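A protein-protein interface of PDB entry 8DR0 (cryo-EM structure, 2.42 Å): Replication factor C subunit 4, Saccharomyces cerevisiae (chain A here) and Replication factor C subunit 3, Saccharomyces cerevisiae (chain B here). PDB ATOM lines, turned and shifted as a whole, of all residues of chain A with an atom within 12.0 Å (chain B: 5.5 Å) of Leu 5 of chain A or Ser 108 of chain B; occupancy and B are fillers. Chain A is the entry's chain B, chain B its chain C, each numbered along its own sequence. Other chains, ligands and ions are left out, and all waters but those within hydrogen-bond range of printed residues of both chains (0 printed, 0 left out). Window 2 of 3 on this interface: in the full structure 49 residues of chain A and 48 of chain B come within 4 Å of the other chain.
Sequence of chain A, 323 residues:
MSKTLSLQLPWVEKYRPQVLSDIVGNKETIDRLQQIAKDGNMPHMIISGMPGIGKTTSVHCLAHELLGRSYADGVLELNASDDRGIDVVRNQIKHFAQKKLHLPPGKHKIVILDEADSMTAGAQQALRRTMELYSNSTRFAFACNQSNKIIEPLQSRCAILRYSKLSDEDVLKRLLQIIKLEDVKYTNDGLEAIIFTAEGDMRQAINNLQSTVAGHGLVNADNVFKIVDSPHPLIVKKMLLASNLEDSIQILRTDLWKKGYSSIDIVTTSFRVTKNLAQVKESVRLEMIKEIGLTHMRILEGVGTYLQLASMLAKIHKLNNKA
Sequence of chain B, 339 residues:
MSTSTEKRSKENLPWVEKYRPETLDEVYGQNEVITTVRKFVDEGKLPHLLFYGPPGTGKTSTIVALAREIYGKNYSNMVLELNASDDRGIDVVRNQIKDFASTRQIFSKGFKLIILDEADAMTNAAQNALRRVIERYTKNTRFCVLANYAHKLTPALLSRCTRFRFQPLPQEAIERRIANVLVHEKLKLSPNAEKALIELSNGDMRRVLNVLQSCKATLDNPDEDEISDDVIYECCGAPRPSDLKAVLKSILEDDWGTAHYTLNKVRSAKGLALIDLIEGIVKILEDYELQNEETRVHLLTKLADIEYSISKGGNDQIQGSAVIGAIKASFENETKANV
The side-chain hydroxyl (OH) of Tyr 71 of chain B lies within hydrogen-bond range of the backbone carbonyl oxygen (O) of Phe 111 of chain B. The side-chain amide nitrogen of Gln 105 of chain B is in hydrogen-bond range of the backbone carbonyl oxygen of Phe 111 of chain B. The side-chain hydroxyl (OG) of Ser 108 of chain B sits at hydrogen-bond distance from the backbone NH (N) of Gly 110 of chain B.
Thr 4 of chain A touches Phe 111 of chain B (O to CE1, 3.5 Å). Ile 70 of chain B touches Leu 5 of chain A (O to CD2, 3.7 Å). Ser 108 of chain B touches Leu 5 of chain A. Gly 110 of chain B touches Leu 5 of chain A. Leu 5 of chain A touches Phe 111 of chain B (O to CD1, 3.3 Å). CB of Phe 111 of chain B touches CD1 of Leu 7 of chain A (3.3 Å).
Of the printed residues of chain B, Thr 4 of chain A touches Phe 111 (3.5 Å). Leu 5 of chain A touches just these residues of chain B: Ile 70 (3.7 Å), Ser 108 (3.9 Å), Gly 110 (3.6 Å) and Phe 111 (3.3 Å). Printed residues of chain B within 4 Å of Leu 7 of chain A: Phe 111. Of the printed residues of chain A, Ile 70 of chain B touches Leu 5 (3.7 Å). No residue of chain A comes within 4 Å of Tyr 71 of chain B. Gln 105 of chain B touches none of the printed residues of chain A. Ser 108 of chain B touches just one residue of chain A: Leu 5. No residue of chain A comes within 4 Å of Lys 109 of chain B. Of chain A, only Leu 5 (3.6 Å) comes within 4 Å of Gly 110 of chain B. Of chain A, only Thr 4 (3.5 Å), Leu 5 (3.3 Å) and Leu 7 (3.3 Å) come within 4 Å of Phe 111 of chain B.
Along chain B the printed residues that touch a printed residue of chain A span positions 70 to 111. Among the printed residues, 6 pairs touch across the chains.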
ATOM      1  N   THR A   4      22.171  -0.473  12.186  1.00  0.00           N
ATOM      2  CA  THR A   4      21.437  -1.717  11.992  1.00  0.00           C
ATOM      3  C   THR A   4      20.343  -1.856  13.046  1.00  0.00           C
ATOM      4  O   THR A   4      20.598  -1.711  14.242  1.00  0.00           O
ATOM      5  CB  THR A   4      22.374  -2.938  12.056  1.00  0.00           C
ATOM      6  OG1 THR A   4      23.161  -3.003  10.861  1.00  0.00           O
ATOM      7  CG2 THR A   4      21.576  -4.226  12.202  1.00  0.00           C
ATOM      8  N   LEU A   5      19.125  -2.141  12.591  1.00  0.00           N
ATOM      9  CA  LEU A   5      17.960  -2.222  13.459  1.00  0.00           C
ATOM     10  C   LEU A   5      17.670  -3.643  13.931  1.00  0.00           C
ATOM     11  O   LEU A   5      16.693  -3.856  14.654  1.00  0.00           O
ATOM     12  CB  LEU A   5      16.736  -1.655  12.737  1.00  0.00           C
ATOM     13  CG  LEU A   5      16.811  -0.185  12.310  1.00  0.00           C
ATOM     14  CD1 LEU A   5      15.448   0.301  11.844  1.00  0.00           C
ATOM     15  CD2 LEU A   5      17.335   0.698  13.433  1.00  0.00           C
ATOM     16  N   SER A   6      18.491  -4.613  13.541  1.00  0.00           N
ATOM     17  CA  SER A   6      18.308  -5.995  13.960  1.00  0.00           C
ATOM     18  C   SER A   6      18.971  -6.238  15.313  1.00  0.00           C
ATOM     19  O   SER A   6      19.905  -5.540  15.712  1.00  0.00           O
ATOM     20  CB  SER A   6      18.885  -6.952  12.917  1.00  0.00           C
ATOM     21  OG  SER A   6      19.389  -8.127  13.529  1.00  0.00           O
ATOM     22  N   LEU A   7      18.465  -7.246  16.022  1.00  0.00           N
ATOM     23  CA  LEU A   7      18.999  -7.644  17.316  1.00  0.00           C
ATOM     24  C   LEU A   7      19.172  -9.155  17.341  1.00  0.00           C
ATOM     25  O   LEU A   7      18.251  -9.894  16.978  1.00  0.00           O
ATOM     26  CB  LEU A   7      18.076  -7.206  18.461  1.00  0.00           C
ATOM     27  CG  LEU A   7      18.327  -5.842  19.111  1.00  0.00           C
ATOM     28  CD1 LEU A   7      17.377  -5.640  20.282  1.00  0.00           C
ATOM     29  CD2 LEU A   7      19.769  -5.686  19.568  1.00  0.00           C
ATOM     30  N   GLN A   8      20.346  -9.609  17.769  1.00  0.00           N
ATOM     31  CA  GLN A   8      20.610 -11.030  17.946  1.00  0.00           C
ATOM     32  C   GLN A   8      20.145 -11.450  19.334  1.00  0.00           C
ATOM     33  O   GLN A   8      20.468 -10.792  20.328  1.00  0.00           O
ATOM     34  CB  GLN A   8      22.100 -11.329  17.758  1.00  0.00           C
ATOM     35  CG  GLN A   8      22.565 -12.678  18.301  1.00  0.00           C
ATOM     36  CD  GLN A   8      24.066 -12.857  18.202  1.00  0.00           C
ATOM     37  OE1 GLN A   8      24.793 -12.653  19.174  1.00  0.00           O
ATOM     38  NE2 GLN A   8      24.541 -13.241  17.023  1.00  0.00           N
ATOM     39  N   LEU A   9      19.389 -12.538  19.398  1.00  0.00           N
ATOM     40  CA  LEU A   9      18.846 -12.986  20.670  1.00  0.00           C
ATOM     41  C   LEU A   9      19.984 -13.390  21.606  1.00  0.00           C
ATOM     42  O   LEU A   9      20.853 -14.178  21.208  1.00  0.00           O
ATOM     43  CB  LEU A   9      17.893 -14.161  20.460  1.00  0.00           C
ATOM     44  CG  LEU A   9      17.052 -14.561  21.675  1.00  0.00           C
ATOM     45  CD1 LEU A   9      16.046 -13.474  22.022  1.00  0.00           C
ATOM     46  CD2 LEU A   9      16.346 -15.884  21.426  1.00  0.00           C
ATOM     47  N   ILE B  70      22.618   4.380  15.310  1.00  0.00           N
ATOM     48  CA  ILE B  70      21.599   3.352  15.123  1.00  0.00           C
ATOM     49  C   ILE B  70      20.361   3.928  14.445  1.00  0.00           C
ATOM     50  O   ILE B  70      19.899   3.409  13.423  1.00  0.00           O
ATOM     51  CB  ILE B  70      21.245   2.699  16.472  1.00  0.00           C
ATOM     52  CG1 ILE B  70      22.445   1.930  17.028  1.00  0.00           C
ATOM     53  CG2 ILE B  70      20.047   1.775  16.317  1.00  0.00           C
ATOM     54  CD1 ILE B  70      22.396   1.735  18.526  1.00  0.00           C
ATOM     55  N   TYR B  71      19.805   5.007  14.997  1.00  0.00           N
ATOM     56  CA  TYR B  71      18.509   5.513  14.562  1.00  0.00           C
ATOM     57  C   TYR B  71      18.602   6.677  13.585  1.00  0.00           C
ATOM     58  O   TYR B  71      17.714   6.828  12.742  1.00  0.00           O
ATOM     59  CB  TYR B  71      17.683   5.949  15.777  1.00  0.00           C
ATOM     60  CG  TYR B  71      17.401   4.826  16.747  1.00  0.00           C
ATOM     61  CD1 TYR B  71      16.450   3.856  16.460  1.00  0.00           C
ATOM     62  CD2 TYR B  71      18.092   4.730  17.947  1.00  0.00           C
ATOM     63  CE1 TYR B  71      16.191   2.826  17.342  1.00  0.00           C
ATOM     64  CE2 TYR B  71      17.841   3.702  18.835  1.00  0.00           C
ATOM     65  CZ  TYR B  71      16.889   2.755  18.528  1.00  0.00           C
ATOM     66  OH  TYR B  71      16.636   1.730  19.409  1.00  0.00           O
ATOM     67  N   MET B  78      13.089   8.050  19.412  1.00  0.00           N
ATOM     68  CA  MET B  78      13.154   6.600  19.305  1.00  0.00           C
ATOM     69  C   MET B  78      13.867   5.944  20.478  1.00  0.00           C
ATOM     70  O   MET B  78      13.976   4.712  20.503  1.00  0.00           O
ATOM     71  CB  MET B  78      13.850   6.203  17.996  1.00  0.00           C
ATOM     72  CG  MET B  78      13.256   6.874  16.765  1.00  0.00           C
ATOM     73  SD  MET B  78      13.980   6.309  15.215  1.00  0.00           S
ATOM     74  CE  MET B  78      13.411   4.613  15.161  1.00  0.00           C
ATOM     75  N   GLN B 105       8.122   0.533  18.157  1.00  0.00           N
ATOM     76  CA  GLN B 105       8.465   1.903  17.799  1.00  0.00           C
ATOM     77  C   GLN B 105       7.355   2.526  16.964  1.00  0.00           C
ATOM     78  O   GLN B 105       6.755   1.868  16.109  1.00  0.00           O
ATOM     79  CB  GLN B 105       9.780   1.940  17.020  1.00  0.00           C
ATOM     80  CG  GLN B 105      11.002   1.525  17.821  1.00  0.00           C
ATOM     81  CD  GLN B 105      11.689   2.699  18.492  1.00  0.00           C
ATOM     82  OE1 GLN B 105      11.111   3.775  18.632  1.00  0.00           O
ATOM     83  NE2 GLN B 105      12.934   2.496  18.905  1.00  0.00           N
ATOM     84  N   ILE B 106       7.079   3.805  17.218  1.00  0.00           N
ATOM     85  CA  ILE B 106       6.078   4.516  16.429  1.00  0.00           C
ATOM     86  C   ILE B 106       6.588   4.755  15.013  1.00  0.00           C
ATOM     87  O   ILE B 106       5.875   4.524  14.030  1.00  0.00           O
ATOM     88  CB  ILE B 106       5.696   5.841  17.113  1.00  0.00           C
ATOM     89  CG1 ILE B 106       5.171   5.590  18.528  1.00  0.00           C
ATOM     90  CG2 ILE B 106       4.655   6.583  16.285  1.00  0.00           C
ATOM     91  CD1 ILE B 106       5.060   6.845  19.362  1.00  0.00           C
ATOM     92  N   PHE B 107       7.832   5.220  14.888  1.00  0.00           N
ATOM     93  CA  PHE B 107       8.340   5.666  13.596  1.00  0.00           C
ATOM     94  C   PHE B 107       8.876   4.505  12.764  1.00  0.00           C
ATOM     95  O   PHE B 107       8.364   4.221  11.675  1.00  0.00           O
ATOM     96  CB  PHE B 107       9.422   6.729  13.810  1.00  0.00           C
ATOM     97  CG  PHE B 107       8.949   7.919  14.597  1.00  0.00           C
ATOM     98  CD1 PHE B 107       8.977   7.908  15.981  1.00  0.00           C
ATOM     99  CD2 PHE B 107       8.464   9.044  13.952  1.00  0.00           C
ATOM    100  CE1 PHE B 107       8.538   8.999  16.706  1.00  0.00           C
ATOM    101  CE2 PHE B 107       8.025  10.138  14.672  1.00  0.00           C
ATOM    102  CZ  PHE B 107       8.062  10.115  16.051  1.00  0.00           C
ATOM    103  N   SER B 108       9.902   3.821  13.260  1.00  0.00           N
ATOM    104  CA  SER B 108      10.559   2.754  12.524  1.00  0.00           C
ATOM    105  C   SER B 108      10.100   1.394  13.047  1.00  0.00           C
ATOM    106  O   SER B 108       9.188   1.292  13.872  1.00  0.00           O
ATOM    107  CB  SER B 108      12.078   2.908  12.623  1.00  0.00           C
ATOM    108  OG  SER B 108      12.593   2.167  13.715  1.00  0.00           O
ATOM    109  N   LYS B 109      10.738   0.332  12.554  1.00  0.00           N
ATOM    110  CA  LYS B 109      10.440  -1.035  12.964  1.00  0.00           C
ATOM    111  C   LYS B 109      11.613  -1.685  13.691  1.00  0.00           C
ATOM    112  O   LYS B 109      11.642  -2.910  13.842  1.00  0.00           O
ATOM    113  CB  LYS B 109      10.047  -1.878  11.749  1.00  0.00           C
ATOM    114  CG  LYS B 109       9.167  -1.160  10.731  1.00  0.00           C
ATOM    115  CD  LYS B 109       7.830  -0.742  11.325  1.00  0.00           C
ATOM    116  CE  LYS B 109       7.163   0.337  10.486  1.00  0.00           C
ATOM    117  NZ  LYS B 109       5.972   0.913  11.167  1.00  0.00           N
ATOM    118  N   GLY B 110      12.579  -0.888  14.150  1.00  0.00           N
ATOM    119  CA  GLY B 110      13.759  -1.415  14.801  1.00  0.00           C
ATOM    120  C   GLY B 110      13.548  -1.671  16.282  1.00  0.00           C
ATOM    121  O   GLY B 110      12.452  -1.540  16.823  1.00  0.00           O
ATOM    122  N   PHE B 111      14.638  -2.053  16.941  1.00  0.00           N
ATOM    123  CA  PHE B 111      14.602  -2.302  18.371  1.00  0.00           C
ATOM    124  C   PHE B 111      14.579  -0.980  19.135  1.00  0.00           C
ATOM    125  O   PHE B 111      14.694   0.106  18.561  1.00  0.00           O
ATOM    126  CB  PHE B 111      15.795  -3.160  18.797  1.00  0.00           C
ATOM    127  CG  PHE B 111      17.123  -2.469  18.666  1.00  0.00           C
ATOM    128  CD1 PHE B 111      17.860  -2.571  17.499  1.00  0.00           C
ATOM    129  CD2 PHE B 111      17.644  -1.737  19.718  1.00  0.00           C
ATOM    130  CE1 PHE B 111      19.084  -1.943  17.380  1.00  0.00           C
ATOM    131  CE2 PHE B 111      18.867  -1.107  19.604  1.00  0.00           C
ATOM    132  CZ  PHE B 111      19.588  -1.211  18.434  1.00  0.00           C
